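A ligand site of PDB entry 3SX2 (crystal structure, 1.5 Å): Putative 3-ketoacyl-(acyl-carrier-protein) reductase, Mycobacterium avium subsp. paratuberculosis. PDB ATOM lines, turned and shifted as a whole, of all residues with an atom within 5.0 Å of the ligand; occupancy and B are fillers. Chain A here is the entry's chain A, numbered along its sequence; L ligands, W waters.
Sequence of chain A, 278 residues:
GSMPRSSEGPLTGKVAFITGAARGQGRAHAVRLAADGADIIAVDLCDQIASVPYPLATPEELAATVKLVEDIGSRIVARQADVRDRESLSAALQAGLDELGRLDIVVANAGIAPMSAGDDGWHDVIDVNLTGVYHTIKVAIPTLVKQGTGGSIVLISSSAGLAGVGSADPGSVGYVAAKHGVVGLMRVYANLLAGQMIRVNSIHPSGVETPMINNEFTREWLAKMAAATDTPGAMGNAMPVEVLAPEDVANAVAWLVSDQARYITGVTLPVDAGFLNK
Merely in contact with the ligand: Ser 206 (3.3 Å), Pro 205 (3.3 Å), Ser 157 (3.3 Å), Gly 207 (3.3 Å), Ala 81 (3.4 Å), Pro 211 (3.4 Å), Gly 20 (3.5 Å), Met 212 (3.5 Å), Ile 112 (3.5 Å), Gly 111 (3.6 Å), Ile 213 (3.6 Å), Ala 110 (3.6 Å), Gly 24 (3.6 Å), Ile 156 (3.7 Å), Leu 56 (3.7 Å), Val 128 (3.7 Å), Ser 158 (3.9 Å), Arg 84 (3.9 Å) and Ala 22 (3.98 Å). Of the 37 residues printed, 31 come within 4 Å of the ligand. The nearest printed residue that does not touch the ligand is Tyr 54 (4.005 Å).
O of Asn 109 is in hydrogen-bond range of O12 of the ligand (2.9 Å). N of Ala 57 lies within hydrogen-bond range of O6 of the ligand, at 3.1 Å. The backbone NH of Gln 25 sits at hydrogen-bond distance from an oxygen (O9) of the ligand (2.8 Å). OD2 of Asp 44 sits at hydrogen-bond distance from O5 of the ligand (2.7 Å). A nitrogen (N3) of the ligand lies within hydrogen-bond range of the side-chain carboxylate of Asp 82 (2.9 Å). An oxygen (O12) of the ligand is in hydrogen-bond range of the side-chain amino group (NZ) of Lys 179, 2.9 Å away. O of Val 208 lies within hydrogen-bond range of N7 of the ligand, at 3.3 Å. The backbone NH (N) of Leu 45 lies within hydrogen-bond range of a nitrogen (N5) of the ligand, 3.1 Å away. The side-chain amide oxygen (OE1) of Gln 25 sits close to an oxygen (O8) of the ligand. OG1 of Thr 210 sits at hydrogen-bond distance from O8 of the ligand (2.8 Å). OH of Tyr 175 is in hydrogen-bond range of O13 of the ligand (2.8 Å). The guanidinium group of Arg 23 lies within salt-bridge range of an oxygen (O2) of the ligand (2.8 Å). O14 of the ligand lies within hydrogen-bond range of N of Val 208 (2.8 Å). A nitrogen (N4) of the ligand sits at hydrogen-bond distance from the backbone NH of Val 83 (3.1 Å).
The backbone carbonyl oxygen (O) of Lys 179 lies within hydrogen-bond range of the side-chain hydroxyl (OG) of Ser 157. The backbone NH of Ile 112 lies within hydrogen-bond range of the side-chain amide oxygen of Asn 129 (2.9 Å). O of Gly 20 lies within hydrogen-bond range of ND2 of Asn 109. OD1 of Asp 44 is in hydrogen-bond range of N of Cys 46 (3.1 Å). N of Ala 81 sits at hydrogen-bond distance from O of Asp 44 (3.0 Å). The side-chain carboxylate (OD2) of Asp 82 is in salt-bridge range of the guanidinium group (NH2) of Arg 84 (2.8 Å). The side-chain amino group (NZ) of Lys 179 is in hydrogen-bond range of the backbone carbonyl oxygen (O) of Ile 156 (3.0 Å). The guanidinium group (NH1) of Arg 23 lies close to the backbone carbonyl oxygen (O) of Leu 56 (3.4 Å).
Water W1 lies within hydrogen-bond range of the side-chain hydroxyl of Tyr 54, an oxygen (O1) of the ligand and the backbone carbonyl oxygen of Gly 111. Water W2 lies within hydrogen-bond range of the side-chain hydroxyl of Tyr 175 and the side-chain hydroxyl of Ser 158. Water W3 lies within hydrogen-bond range of the side-chain hydroxyl of Ser 158 (2.8 Å) and the backbone carbonyl oxygen of Pro 205 (3.3 Å).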
ATOM      1  N   GLY A  20      -8.253  -4.953 -17.445  1.00  0.00           N
ATOM      2  CA  GLY A  20      -6.825  -4.736 -17.617  1.00  0.00           C
ATOM      3  C   GLY A  20      -6.486  -3.686 -18.643  1.00  0.00           C
ATOM      4  O   GLY A  20      -5.514  -3.835 -19.407  1.00  0.00           O
ATOM      5  N   ALA A  22      -5.364  -0.590 -18.396  1.00  0.00           N
ATOM      6  CA  ALA A  22      -4.438   0.493 -18.095  1.00  0.00           C
ATOM      7  C   ALA A  22      -3.224   0.557 -18.995  1.00  0.00           C
ATOM      8  O   ALA A  22      -2.612   1.618 -19.155  1.00  0.00           O
ATOM      9  CB  ALA A  22      -3.981   0.441 -16.647  1.00  0.00           C
ATOM     10  N   ARG A  23      -2.855  -0.548 -19.600  1.00  0.00           N
ATOM     11  CA  ARG A  23      -1.643  -0.609 -20.420  1.00  0.00           C
ATOM     12  C   ARG A  23      -1.682  -1.851 -21.284  1.00  0.00           C
ATOM     13  O   ARG A  23      -2.650  -2.631 -21.253  1.00  0.00           O
ATOM     14  CB  ARG A  23      -0.399  -0.590 -19.545  1.00  0.00           C
ATOM     15  CG  ARG A  23      -0.179  -1.913 -18.791  1.00  0.00           C
ATOM     16  CD  ARG A  23       1.139  -1.932 -18.015  1.00  0.00           C
ATOM     17  NE  ARG A  23       1.414  -3.280 -17.564  1.00  0.00           N
ATOM     18  CZ  ARG A  23       2.156  -3.589 -16.513  1.00  0.00           C
ATOM     19  NH1 ARG A  23       2.716  -2.640 -15.789  1.00  0.00           N
ATOM     20  NH2 ARG A  23       2.242  -4.879 -16.120  1.00  0.00           N
ATOM     21  N   GLY A  24      -0.603  -2.077 -22.019  1.00  0.00           N
ATOM     22  CA  GLY A  24      -0.444  -3.341 -22.690  1.00  0.00           C
ATOM     23  C   GLY A  24      -1.534  -3.663 -23.686  1.00  0.00           C
ATOM     24  O   GLY A  24      -2.011  -2.802 -24.431  1.00  0.00           O
ATOM     25  N   GLN A  25      -1.915  -4.925 -23.735  1.00  0.00           N
ATOM     26  CA  GLN A  25      -2.956  -5.324 -24.678  1.00  0.00           C
ATOM     27  C   GLN A  25      -4.303  -4.665 -24.410  1.00  0.00           C
ATOM     28  O   GLN A  25      -5.037  -4.320 -25.327  1.00  0.00           O
ATOM     29  CB  GLN A  25      -3.118  -6.868 -24.720  1.00  0.00           C
ATOM     30  CG  GLN A  25      -1.858  -7.549 -25.243  1.00  0.00           C
ATOM     31  CD  GLN A  25      -1.914  -9.071 -25.167  1.00  0.00           C
ATOM     32  OE1 GLN A  25      -1.097  -9.704 -24.419  1.00  0.00           O
ATOM     33  NE2 GLN A  25      -2.827  -9.640 -25.866  1.00  0.00           N
ATOM     34  N   GLY A  26      -4.662  -4.517 -23.138  1.00  0.00           N
ATOM     35  CA  GLY A  26      -5.928  -3.936 -22.753  1.00  0.00           C
ATOM     36  C   GLY A  26      -6.052  -2.486 -23.237  1.00  0.00           C
ATOM     37  O   GLY A  26      -7.068  -2.086 -23.788  1.00  0.00           O
ATOM     38  N   VAL A  43     -11.424  -0.911 -17.015  1.00  0.00           N
ATOM     39  CA  VAL A  43     -11.104  -1.191 -15.617  1.00  0.00           C
ATOM     40  C   VAL A  43      -9.712  -1.768 -15.492  1.00  0.00           C
ATOM     41  O   VAL A  43      -9.234  -2.492 -16.379  1.00  0.00           O
ATOM     42  CB  VAL A  43     -12.127  -2.073 -14.878  1.00  0.00           C
ATOM     43  CG1 VAL A  43     -13.566  -1.479 -14.964  1.00  0.00           C
ATOM     44  CG2 VAL A  43     -12.122  -3.450 -15.388  1.00  0.00           C
ATOM     45  N   ASP A  44      -9.063  -1.482 -14.365  1.00  0.00           N
ATOM     46  CA  ASP A  44      -7.763  -2.041 -14.039  1.00  0.00           C
ATOM     47  C   ASP A  44      -7.560  -2.017 -12.554  1.00  0.00           C
ATOM     48  O   ASP A  44      -8.050  -1.132 -11.865  1.00  0.00           O
ATOM     49  CB  ASP A  44      -6.644  -1.261 -14.736  1.00  0.00           C
ATOM     50  CG  ASP A  44      -5.383  -2.088 -14.933  1.00  0.00           C
ATOM     51  OD1 ASP A  44      -4.644  -2.295 -13.940  1.00  0.00           O
ATOM     52  OD2 ASP A  44      -5.142  -2.544 -16.079  1.00  0.00           O
ATOM     53  N   LEU A  45      -6.775  -2.944 -12.046  1.00  0.00           N
ATOM     54  CA  LEU A  45      -6.421  -2.984 -10.630  1.00  0.00           C
ATOM     55  C   LEU A  45      -5.609  -1.779 -10.196  1.00  0.00           C
ATOM     56  O   LEU A  45      -5.766  -1.295  -9.090  1.00  0.00           O
ATOM     57  CB  LEU A  45      -5.655  -4.290 -10.330  1.00  0.00           C
ATOM     58  CG  LEU A  45      -5.249  -4.542  -8.907  1.00  0.00           C
ATOM     59  CD1 LEU A  45      -6.475  -4.741  -8.037  1.00  0.00           C
ATOM     60  CD2 LEU A  45      -4.404  -5.782  -8.798  1.00  0.00           C
ATOM     61  N   CYS A  46      -4.670  -1.345 -11.031  1.00  0.00           N
ATOM     62  CA  CYS A  46      -3.824  -0.194 -10.712  1.00  0.00           C
ATOM     63  C   CYS A  46      -3.140  -0.335  -9.342  1.00  0.00           C
ATOM     64  O   CYS A  46      -2.971   0.635  -8.584  1.00  0.00           O
ATOM     65  CB  CYS A  46      -4.591   1.128 -10.770  1.00  0.00           C
ATOM     66  SG  CYS A  46      -5.350   1.496 -12.375  1.00  0.00           S
ATOM     67  N   ILE A  49       0.158  -6.995  -7.038  1.00  0.00           N
ATOM     68  CA  ILE A  49      -0.068  -8.301  -6.403  1.00  0.00           C
ATOM     69  C   ILE A  49       1.309  -8.849  -6.066  1.00  0.00           C
ATOM     70  O   ILE A  49       2.199  -8.870  -6.943  1.00  0.00           O
ATOM     71  CB  ILE A  49      -0.893  -9.222  -7.315  1.00  0.00           C
ATOM     72  CG1 ILE A  49      -2.304  -8.641  -7.532  1.00  0.00           C
ATOM     73  CG2 ILE A  49      -0.938 -10.678  -6.772  1.00  0.00           C
ATOM     74  CD1 ILE A  49      -3.171  -9.396  -8.548  1.00  0.00           C
ATOM     75  N   TYR A  54       6.996  -8.441 -11.640  1.00  0.00           N
ATOM     76  CA  TYR A  54       7.140  -7.231 -12.482  1.00  0.00           C
ATOM     77  C   TYR A  54       6.018  -6.304 -12.007  1.00  0.00           C
ATOM     78  O   TYR A  54       5.026  -6.775 -11.404  1.00  0.00           O
ATOM     79  CB  TYR A  54       7.013  -7.563 -14.002  1.00  0.00           C
ATOM     80  CG  TYR A  54       5.715  -8.270 -14.340  1.00  0.00           C
ATOM     81  CD1 TYR A  54       5.649  -9.668 -14.334  1.00  0.00           C
ATOM     82  CD2 TYR A  54       4.587  -7.576 -14.604  1.00  0.00           C
ATOM     83  CE1 TYR A  54       4.457 -10.328 -14.601  1.00  0.00           C
ATOM     84  CE2 TYR A  54       3.388  -8.195 -14.845  1.00  0.00           C
ATOM     85  CZ  TYR A  54       3.333  -9.605 -14.832  1.00  0.00           C
ATOM     86  OH  TYR A  54       2.127 -10.248 -15.035  1.00  0.00           O
ATOM     87  N   LEU A  56       2.696  -4.236 -11.830  1.00  0.00           N
ATOM     88  CA  LEU A  56       1.377  -4.075 -12.442  1.00  0.00           C
ATOM     89  C   LEU A  56       1.128  -2.586 -12.754  1.00  0.00           C
ATOM     90  O   LEU A  56       2.011  -1.745 -12.544  1.00  0.00           O
ATOM     91  CB  LEU A  56       0.270  -4.695 -11.584  1.00  0.00           C
ATOM     92  CG  LEU A  56       0.413  -6.209 -11.307  1.00  0.00           C
ATOM     93  CD1 LEU A  56      -0.840  -6.716 -10.612  1.00  0.00           C
ATOM     94  CD2 LEU A  56       0.747  -6.959 -12.603  1.00  0.00           C
ATOM     95  N   ALA A  57      -0.001  -2.263 -13.392  1.00  0.00           N
ATOM     96  CA  ALA A  57      -0.235  -0.890 -13.898  1.00  0.00           C
ATOM     97  C   ALA A  57      -0.369   0.065 -12.742  1.00  0.00           C
ATOM     98  O   ALA A  57      -0.777  -0.312 -11.635  1.00  0.00           O
ATOM     99  CB  ALA A  57      -1.519  -0.832 -14.753  1.00  0.00           C
ATOM    100  N   ALA A  81     -10.617  -1.360 -10.409  1.00  0.00           N
ATOM    101  CA  ALA A  81     -11.412  -2.492  -9.989  1.00  0.00           C
ATOM    102  C   ALA A  81     -10.553  -3.739 -10.056  1.00  0.00           C
ATOM    103  O   ALA A  81      -9.594  -3.796 -10.839  1.00  0.00           O
ATOM    104  CB  ALA A  81     -12.663  -2.644 -10.887  1.00  0.00           C
ATOM    105  N   ASP A  82     -10.883  -4.716  -9.241  1.00  0.00           N
ATOM    106  CA  ASP A  82     -10.159  -5.991  -9.154  1.00  0.00           C
ATOM    107  C   ASP A  82     -11.067  -7.079  -9.688  1.00  0.00           C
ATOM    108  O   ASP A  82     -12.128  -7.341  -9.090  1.00  0.00           O
ATOM    109  CB  ASP A  82      -9.746  -6.229  -7.699  1.00  0.00           C
ATOM    110  CG  ASP A  82      -8.846  -7.420  -7.487  1.00  0.00           C
ATOM    111  OD1 ASP A  82      -8.698  -8.296  -8.387  1.00  0.00           O
ATOM    112  OD2 ASP A  82      -8.254  -7.519  -6.369  1.00  0.00           O
ATOM    113  N   VAL A  83     -10.667  -7.760 -10.771  1.00  0.00           N
ATOM    114  CA  VAL A  83     -11.471  -8.844 -11.331  1.00  0.00           C
ATOM    115  C   VAL A  83     -11.719  -9.995 -10.352  1.00  0.00           C
ATOM    116  O   VAL A  83     -12.656 -10.741 -10.519  1.00  0.00           O
ATOM    117  CB  VAL A  83     -10.939  -9.385 -12.696  1.00  0.00           C
ATOM    118  CG1 VAL A  83     -10.960  -8.290 -13.774  1.00  0.00           C
ATOM    119  CG2 VAL A  83      -9.544 -10.018 -12.603  1.00  0.00           C
ATOM    120  N   ARG A  84     -10.853 -10.120  -9.340  1.00  0.00           N
ATOM    121  CA  ARG A  84     -11.028 -11.159  -8.327  1.00  0.00           C
ATOM    122  C   ARG A  84     -12.234 -10.938  -7.435  1.00  0.00           C
ATOM    123  O   ARG A  84     -12.667 -11.894  -6.764  1.00  0.00           O
ATOM    124  CB  ARG A  84      -9.795 -11.230  -7.424  1.00  0.00           C
ATOM    125  CG  ARG A  84      -8.517 -11.721  -8.138  1.00  0.00           C
ATOM    126  CD  ARG A  84      -7.317 -11.662  -7.245  1.00  0.00           C
ATOM    127  NE  ARG A  84      -6.943 -10.290  -6.965  1.00  0.00           N
ATOM    128  CZ  ARG A  84      -5.918  -9.921  -6.193  1.00  0.00           C
ATOM    129  NH1 ARG A  84      -5.154 -10.854  -5.624  1.00  0.00           N
ATOM    130  NH2 ARG A  84      -5.698  -8.650  -5.987  1.00  0.00           N
ATOM    131  N   ASN A 109      -9.501  -9.394 -20.483  1.00  0.00           N
ATOM    132  CA  ASN A 109      -8.072  -9.327 -20.789  1.00  0.00           C
ATOM    133  C   ASN A 109      -7.197  -9.281 -19.533  1.00  0.00           C
ATOM    134  O   ASN A 109      -6.024  -9.657 -19.645  1.00  0.00           O
ATOM    135  CB  ASN A 109      -7.851  -8.097 -21.691  1.00  0.00           C
ATOM    136  CG  ASN A 109      -6.410  -7.639 -21.731  1.00  0.00           C
ATOM    137  OD1 ASN A 109      -5.631  -8.066 -22.565  1.00  0.00           O
ATOM    138  ND2 ASN A 109      -6.078  -6.705 -20.853  1.00  0.00           N
ATOM    139  N   ALA A 110      -7.665  -8.756 -18.386  1.00  0.00           N
ATOM    140  CA  ALA A 110      -6.783  -8.707 -17.204  1.00  0.00           C
ATOM    141  C   ALA A 110      -6.163 -10.054 -16.955  1.00  0.00           C
ATOM    142  O   ALA A 110      -6.844 -11.070 -16.959  1.00  0.00           O
ATOM    143  CB  ALA A 110      -7.521  -8.235 -15.981  1.00  0.00           C
ATOM    144  N   GLY A 111      -4.868 -10.061 -16.650  1.00  0.00           N
ATOM    145  CA  GLY A 111      -4.209 -11.314 -16.291  1.00  0.00           C
ATOM    146  C   GLY A 111      -2.850 -10.992 -15.660  1.00  0.00           C
ATOM    147  O   GLY A 111      -2.314  -9.892 -15.827  1.00  0.00           O
ATOM    148  N   ILE A 112      -2.299 -11.987 -14.968  1.00  0.00           N
ATOM    149  CA  ILE A 112      -1.004 -11.892 -14.331  1.00  0.00           C
ATOM    150  C   ILE A 112      -0.200 -13.154 -14.617  1.00  0.00           C
ATOM    151  O   ILE A 112      -0.740 -14.217 -14.902  1.00  0.00           O
ATOM    152  CB  ILE A 112      -1.074 -11.651 -12.793  1.00  0.00           C
ATOM    153  CG1 ILE A 112      -1.927 -12.731 -12.086  1.00  0.00           C
ATOM    154  CG2 ILE A 112      -1.628 -10.264 -12.471  1.00  0.00           C
ATOM    155  CD1 ILE A 112      -1.815 -12.736 -10.569  1.00  0.00           C
ATOM    156  N   VAL A 128      -7.004 -14.477 -10.522  1.00  0.00           N
ATOM    157  CA  VAL A 128      -7.099 -13.445 -11.550  1.00  0.00           C
ATOM    158  C   VAL A 128      -7.463 -13.998 -12.921  1.00  0.00           C
ATOM    159  O   VAL A 128      -8.388 -13.516 -13.584  1.00  0.00           O
ATOM    160  CB  VAL A 128      -5.777 -12.650 -11.684  1.00  0.00           C
ATOM    161  CG1 VAL A 128      -5.908 -11.589 -12.752  1.00  0.00           C
ATOM    162  CG2 VAL A 128      -5.379 -12.016 -10.318  1.00  0.00           C
ATOM    163  N   ASN A 129      -6.742 -15.029 -13.355  1.00  0.00           N
ATOM    164  CA  ASN A 129      -6.776 -15.473 -14.746  1.00  0.00           C
ATOM    165  C   ASN A 129      -7.912 -16.432 -15.045  1.00  0.00           C
ATOM    166  O   ASN A 129      -8.264 -16.609 -16.216  1.00  0.00           O
ATOM    167  CB  ASN A 129      -5.457 -16.127 -15.220  1.00  0.00           C
ATOM    168  CG  ASN A 129      -4.265 -15.170 -15.228  1.00  0.00           C
ATOM    169  OD1 ASN A 129      -4.314 -14.052 -14.669  1.00  0.00           O
ATOM    170  ND2 ASN A 129      -3.184 -15.578 -15.917  1.00  0.00           N
ATOM    171  N   ILE A 156      -9.344 -13.685 -23.223  1.00  0.00           N
ATOM    172  CA  ILE A 156      -7.918 -13.726 -23.573  1.00  0.00           C
ATOM    173  C   ILE A 156      -7.261 -14.878 -22.865  1.00  0.00           C
ATOM    174  O   ILE A 156      -7.080 -14.867 -21.658  1.00  0.00           O
ATOM    175  CB  ILE A 156      -7.202 -12.402 -23.322  1.00  0.00           C
ATOM    176  CG1 ILE A 156      -7.939 -11.199 -23.913  1.00  0.00           C
ATOM    177  CG2 ILE A 156      -5.718 -12.527 -23.843  1.00  0.00           C
ATOM    178  CD1 ILE A 156      -8.169 -11.251 -25.422  1.00  0.00           C
ATOM    179  N   SER A 157      -6.947 -15.920 -23.637  1.00  0.00           N
ATOM    180  CA  SER A 157      -6.243 -17.078 -23.120  1.00  0.00           C
ATOM    181  C   SER A 157      -4.740 -16.875 -23.478  1.00  0.00           C
ATOM    182  O   SER A 157      -4.213 -15.779 -23.229  1.00  0.00           O
ATOM    183  CB  SER A 157      -6.860 -18.336 -23.678  1.00  0.00           C
ATOM    184  OG  SER A 157      -6.212 -19.499 -23.191  1.00  0.00           O
ATOM    185  N   SER A 158      -4.077 -17.867 -24.057  1.00  0.00           N
ATOM    186  CA  SER A 158      -2.635 -17.884 -24.331  1.00  0.00           C
ATOM    187  C   SER A 158      -2.324 -19.145 -25.125  1.00  0.00           C
ATOM    188  O   SER A 158      -3.119 -20.117 -25.090  1.00  0.00           O
ATOM    189  CB  SER A 158      -1.901 -17.947 -22.981  1.00  0.00           C
ATOM    190  OG  SER A 158      -0.521 -18.251 -23.117  1.00  0.00           O
ATOM    191  N   TYR A 175      -0.715 -20.857 -14.428  1.00  0.00           N
ATOM    192  CA  TYR A 175      -0.989 -20.104 -15.647  1.00  0.00           C
ATOM    193  C   TYR A 175      -1.502 -21.026 -16.744  1.00  0.00           C
ATOM    194  O   TYR A 175      -2.514 -20.725 -17.402  1.00  0.00           O
ATOM    195  CB  TYR A 175       0.272 -19.368 -16.082  1.00  0.00           C
ATOM    196  CG  TYR A 175       0.064 -18.325 -17.173  1.00  0.00           C
ATOM    197  CD1 TYR A 175      -0.176 -16.993 -16.850  1.00  0.00           C
ATOM    198  CD2 TYR A 175       0.110 -18.678 -18.517  1.00  0.00           C
ATOM    199  CE1 TYR A 175      -0.331 -16.034 -17.836  1.00  0.00           C
ATOM    200  CE2 TYR A 175      -0.035 -17.724 -19.525  1.00  0.00           C
ATOM    201  CZ  TYR A 175      -0.269 -16.398 -19.166  1.00  0.00           C
ATOM    202  OH  TYR A 175      -0.377 -15.442 -20.207  1.00  0.00           O
ATOM    203  N   LYS A 179      -5.330 -20.751 -18.031  1.00  0.00           N
ATOM    204  CA  LYS A 179      -5.576 -20.409 -19.440  1.00  0.00           C
ATOM    205  C   LYS A 179      -6.309 -21.531 -20.165  1.00  0.00           C
ATOM    206  O   LYS A 179      -7.102 -21.280 -21.077  1.00  0.00           O
ATOM    207  CB  LYS A 179      -4.241 -20.050 -20.140  1.00  0.00           C
ATOM    208  CG  LYS A 179      -3.636 -18.722 -19.598  1.00  0.00           C
ATOM    209  CD  LYS A 179      -4.533 -17.537 -19.797  1.00  0.00           C
ATOM    210  CE  LYS A 179      -3.799 -16.198 -19.701  1.00  0.00           C
ATOM    211  NZ  LYS A 179      -4.749 -15.057 -19.843  1.00  0.00           N
ATOM    212  N   PRO A 205      -2.674 -15.642 -27.860  1.00  0.00           N
ATOM    213  CA  PRO A 205      -1.377 -15.116 -28.315  1.00  0.00           C
ATOM    214  C   PRO A 205      -0.215 -15.945 -27.811  1.00  0.00           C
ATOM    215  O   PRO A 205      -0.313 -16.566 -26.759  1.00  0.00           O
ATOM    216  CB  PRO A 205      -1.352 -13.697 -27.690  1.00  0.00           C
ATOM    217  CG  PRO A 205      -2.759 -13.407 -27.188  1.00  0.00           C
ATOM    218  CD  PRO A 205      -3.237 -14.804 -26.811  1.00  0.00           C
ATOM    219  N   SER A 206       0.824 -16.026 -28.621  1.00  0.00           N
ATOM    220  CA  SER A 206       2.137 -16.310 -28.102  1.00  0.00           C
ATOM    221  C   SER A 206       2.632 -14.949 -27.603  1.00  0.00           C
ATOM    222  O   SER A 206       1.838 -14.063 -27.307  1.00  0.00           O
ATOM    223  CB  SER A 206       3.010 -17.015 -29.143  1.00  0.00           C
ATOM    224  OG  SER A 206       3.193 -16.204 -30.295  1.00  0.00           O
ATOM    225  N   GLY A 207       3.912 -14.780 -27.537  1.00  0.00           N
ATOM    226  CA  GLY A 207       4.441 -13.687 -26.773  1.00  0.00           C
ATOM    227  C   GLY A 207       4.054 -12.370 -27.402  1.00  0.00           C
ATOM    228  O   GLY A 207       4.146 -12.212 -28.630  1.00  0.00           O
ATOM    229  N   VAL A 208       3.733 -11.388 -26.572  1.00  0.00           N
ATOM    230  CA  VAL A 208       3.278 -10.070 -26.991  1.00  0.00           C
ATOM    231  C   VAL A 208       4.104  -9.065 -26.231  1.00  0.00           C
ATOM    232  O   VAL A 208       4.345  -9.236 -25.042  1.00  0.00           O
ATOM    233  CB  VAL A 208       1.786  -9.870 -26.667  1.00  0.00           C
ATOM    234  CG1 VAL A 208       1.287  -8.510 -27.150  1.00  0.00           C
ATOM    235  CG2 VAL A 208       0.925 -10.958 -27.338  1.00  0.00           C
ATOM    236  N   THR A 210       4.732  -6.538 -24.028  1.00  0.00           N
ATOM    237  CA  THR A 210       4.141  -5.780 -22.926  1.00  0.00           C
ATOM    238  C   THR A 210       4.999  -5.971 -21.689  1.00  0.00           C
ATOM    239  O   THR A 210       5.855  -6.841 -21.677  1.00  0.00           O
ATOM    240  CB  THR A 210       2.715  -6.299 -22.574  1.00  0.00           C
ATOM    241  OG1 THR A 210       2.849  -7.590 -21.953  1.00  0.00           O
ATOM    242  CG2 THR A 210       1.807  -6.382 -23.834  1.00  0.00           C
ATOM    243  N   PRO A 211       4.706  -5.213 -20.609  1.00  0.00           N
ATOM    244  CA  PRO A 211       5.521  -5.362 -19.437  1.00  0.00           C
ATOM    245  C   PRO A 211       5.448  -6.733 -18.763  1.00  0.00           C
ATOM    246  O   PRO A 211       6.298  -7.062 -17.928  1.00  0.00           O
ATOM    247  CB  PRO A 211       4.973  -4.241 -18.525  1.00  0.00           C
ATOM    248  CG  PRO A 211       4.514  -3.248 -19.434  1.00  0.00           C
ATOM    249  CD  PRO A 211       3.877  -3.996 -20.550  1.00  0.00           C
ATOM    250  N   MET A 212       4.426  -7.533 -19.087  1.00  0.00           N
ATOM    251  CA  MET A 212       4.360  -8.899 -18.571  1.00  0.00           C
ATOM    252  C   MET A 212       5.588  -9.721 -18.958  1.00  0.00           C
ATOM    253  O   MET A 212       6.062 -10.534 -18.151  1.00  0.00           O
ATOM    254  CB  MET A 212       3.089  -9.624 -19.053  1.00  0.00           C
ATOM    255  CG  MET A 212       2.980 -11.109 -18.543  1.00  0.00           C
ATOM    256  SD  MET A 212       1.426 -11.881 -19.032  1.00  0.00           S
ATOM    257  CE  MET A 212       0.335 -11.166 -17.852  1.00  0.00           C
ATOM    258  N   ILE A 213       6.117  -9.524 -20.165  1.00  0.00           N
ATOM    259  CA  ILE A 213       7.286 -10.302 -20.602  1.00  0.00           C
ATOM    260  C   ILE A 213       8.502  -9.472 -20.880  1.00  0.00           C
ATOM    261  O   ILE A 213       9.596 -10.028 -20.979  1.00  0.00           O
ATOM    262  CB  ILE A 213       6.983 -11.193 -21.813  1.00  0.00           C
ATOM    263  CG1 ILE A 213       6.673 -10.405 -23.061  1.00  0.00           C
ATOM    264  CG2 ILE A 213       5.843 -12.196 -21.461  1.00  0.00           C
ATOM    265  CD1 ILE A 213       6.644 -11.300 -24.383  1.00  0.00           C
HETATM  266  P1  LIG L   1       0.188  -6.444 -18.806  1.00  0.00           P
HETATM  267  O1  LIG L   1       0.732  -6.879 -17.538  1.00  0.00           O
HETATM  268  O2  LIG L   1       0.908  -5.259 -19.508  1.00  0.00           O
HETATM  269  O3  LIG L   1      -1.375  -6.059 -18.725  1.00  0.00           O
HETATM  270  C1  LIG L   1      -2.269  -6.781 -17.890  1.00  0.00           C
HETATM  271  C2  LIG L   1      -3.086  -5.714 -17.119  1.00  0.00           C
HETATM  272  O4  LIG L   1      -4.036  -6.347 -16.276  1.00  0.00           O
HETATM  273  C3  LIG L   1      -2.363  -4.647 -16.346  1.00  0.00           C
HETATM  274  O5  LIG L   1      -2.629  -3.307 -16.654  1.00  0.00           O
HETATM  275  C4  LIG L   1      -2.607  -5.012 -14.928  1.00  0.00           C
HETATM  276  O6  LIG L   1      -2.516  -4.060 -13.891  1.00  0.00           O
HETATM  277  C5  LIG L   1      -4.007  -5.618 -14.990  1.00  0.00           C
HETATM  278  N1  LIG L   1      -4.469  -6.529 -14.003  1.00  0.00           N
HETATM  279  C6  LIG L   1      -3.744  -7.603 -13.453  1.00  0.00           C
HETATM  280  N2  LIG L   1      -4.462  -8.220 -12.456  1.00  0.00           N
HETATM  281  C7  LIG L   1      -5.649  -7.504 -12.358  1.00  0.00           C
HETATM  282  C8  LIG L   1      -6.781  -7.685 -11.562  1.00  0.00           C
HETATM  283  N3  LIG L   1      -6.826  -8.628 -10.521  1.00  0.00           N
HETATM  284  N4  LIG L   1      -7.865  -6.924 -11.782  1.00  0.00           N
HETATM  285  C9  LIG L   1      -7.814  -5.901 -12.763  1.00  0.00           C
HETATM  286  N5  LIG L   1      -6.754  -5.678 -13.582  1.00  0.00           N
HETATM  287  C10 LIG L   1      -5.683  -6.538 -13.371  1.00  0.00           C
HETATM  288  O7  LIG L   1       0.230  -7.752 -19.770  1.00  0.00           O
HETATM  289  P2  LIG L   1      -0.594  -8.060 -21.129  1.00  0.00           P
HETATM  290  O8  LIG L   1       0.367  -8.785 -21.988  1.00  0.00           O
HETATM  291  O9  LIG L   1      -1.198  -6.781 -21.747  1.00  0.00           O
HETATM  292  O10 LIG L   1      -1.746  -9.057 -20.537  1.00  0.00           O
HETATM  293  C11 LIG L   1      -3.029  -9.048 -21.152  1.00  0.00           C
HETATM  294  C12 LIG L   1      -3.517 -10.481 -21.194  1.00  0.00           C
HETATM  295  O11 LIG L   1      -2.731 -11.172 -22.228  1.00  0.00           O
HETATM  296  C13 LIG L   1      -3.400 -11.367 -19.957  1.00  0.00           C
HETATM  297  O12 LIG L   1      -4.539 -12.163 -19.755  1.00  0.00           O
HETATM  298  C14 LIG L   1      -2.223 -12.198 -20.201  1.00  0.00           C
HETATM  299  O13 LIG L   1      -2.173 -13.396 -19.454  1.00  0.00           O
HETATM  300  C15 LIG L   1      -2.350 -12.466 -21.693  1.00  0.00           C
HETATM  301  N6  LIG L   1      -1.251 -12.976 -22.526  1.00  0.00           N
HETATM  302  C16 LIG L   1      -0.027 -12.230 -22.496  1.00  0.00           C
HETATM  303  C17 LIG L   1       1.012 -12.674 -23.343  1.00  0.00           C
HETATM  304  C18 LIG L   1       2.313 -11.923 -23.396  1.00  0.00           C
HETATM  305  O14 LIG L   1       3.260 -12.402 -23.964  1.00  0.00           O
HETATM  306  N7  LIG L   1       2.321 -10.630 -22.854  1.00  0.00           N
HETATM  307  C19 LIG L   1       0.936 -13.846 -24.174  1.00  0.00           C
HETATM  308  C20 LIG L   1      -0.328 -14.500 -24.200  1.00  0.00           C
HETATM  309  C21 LIG L   1      -1.387 -14.068 -23.346  1.00  0.00           C
HETATM  310  O   HOH W   1       0.096  -8.568 -15.508  1.00  0.00           O
HETATM  311  O   HOH W   2       1.586 -16.235 -21.818  1.00  0.00           O
HETATM  312  O   HOH W   3       1.749 -17.212 -24.328  1.00  0.00           O
HETATM  313  O   HOH W   4      -3.410  -5.496 -20.743  1.00  0.00           O
HETATM  314  O   HOH W   5      -7.564 -12.658 -19.208  1.00  0.00           O
HETATM  315  O   HOH W   6       3.768 -14.859 -22.758  1.00  0.00           O
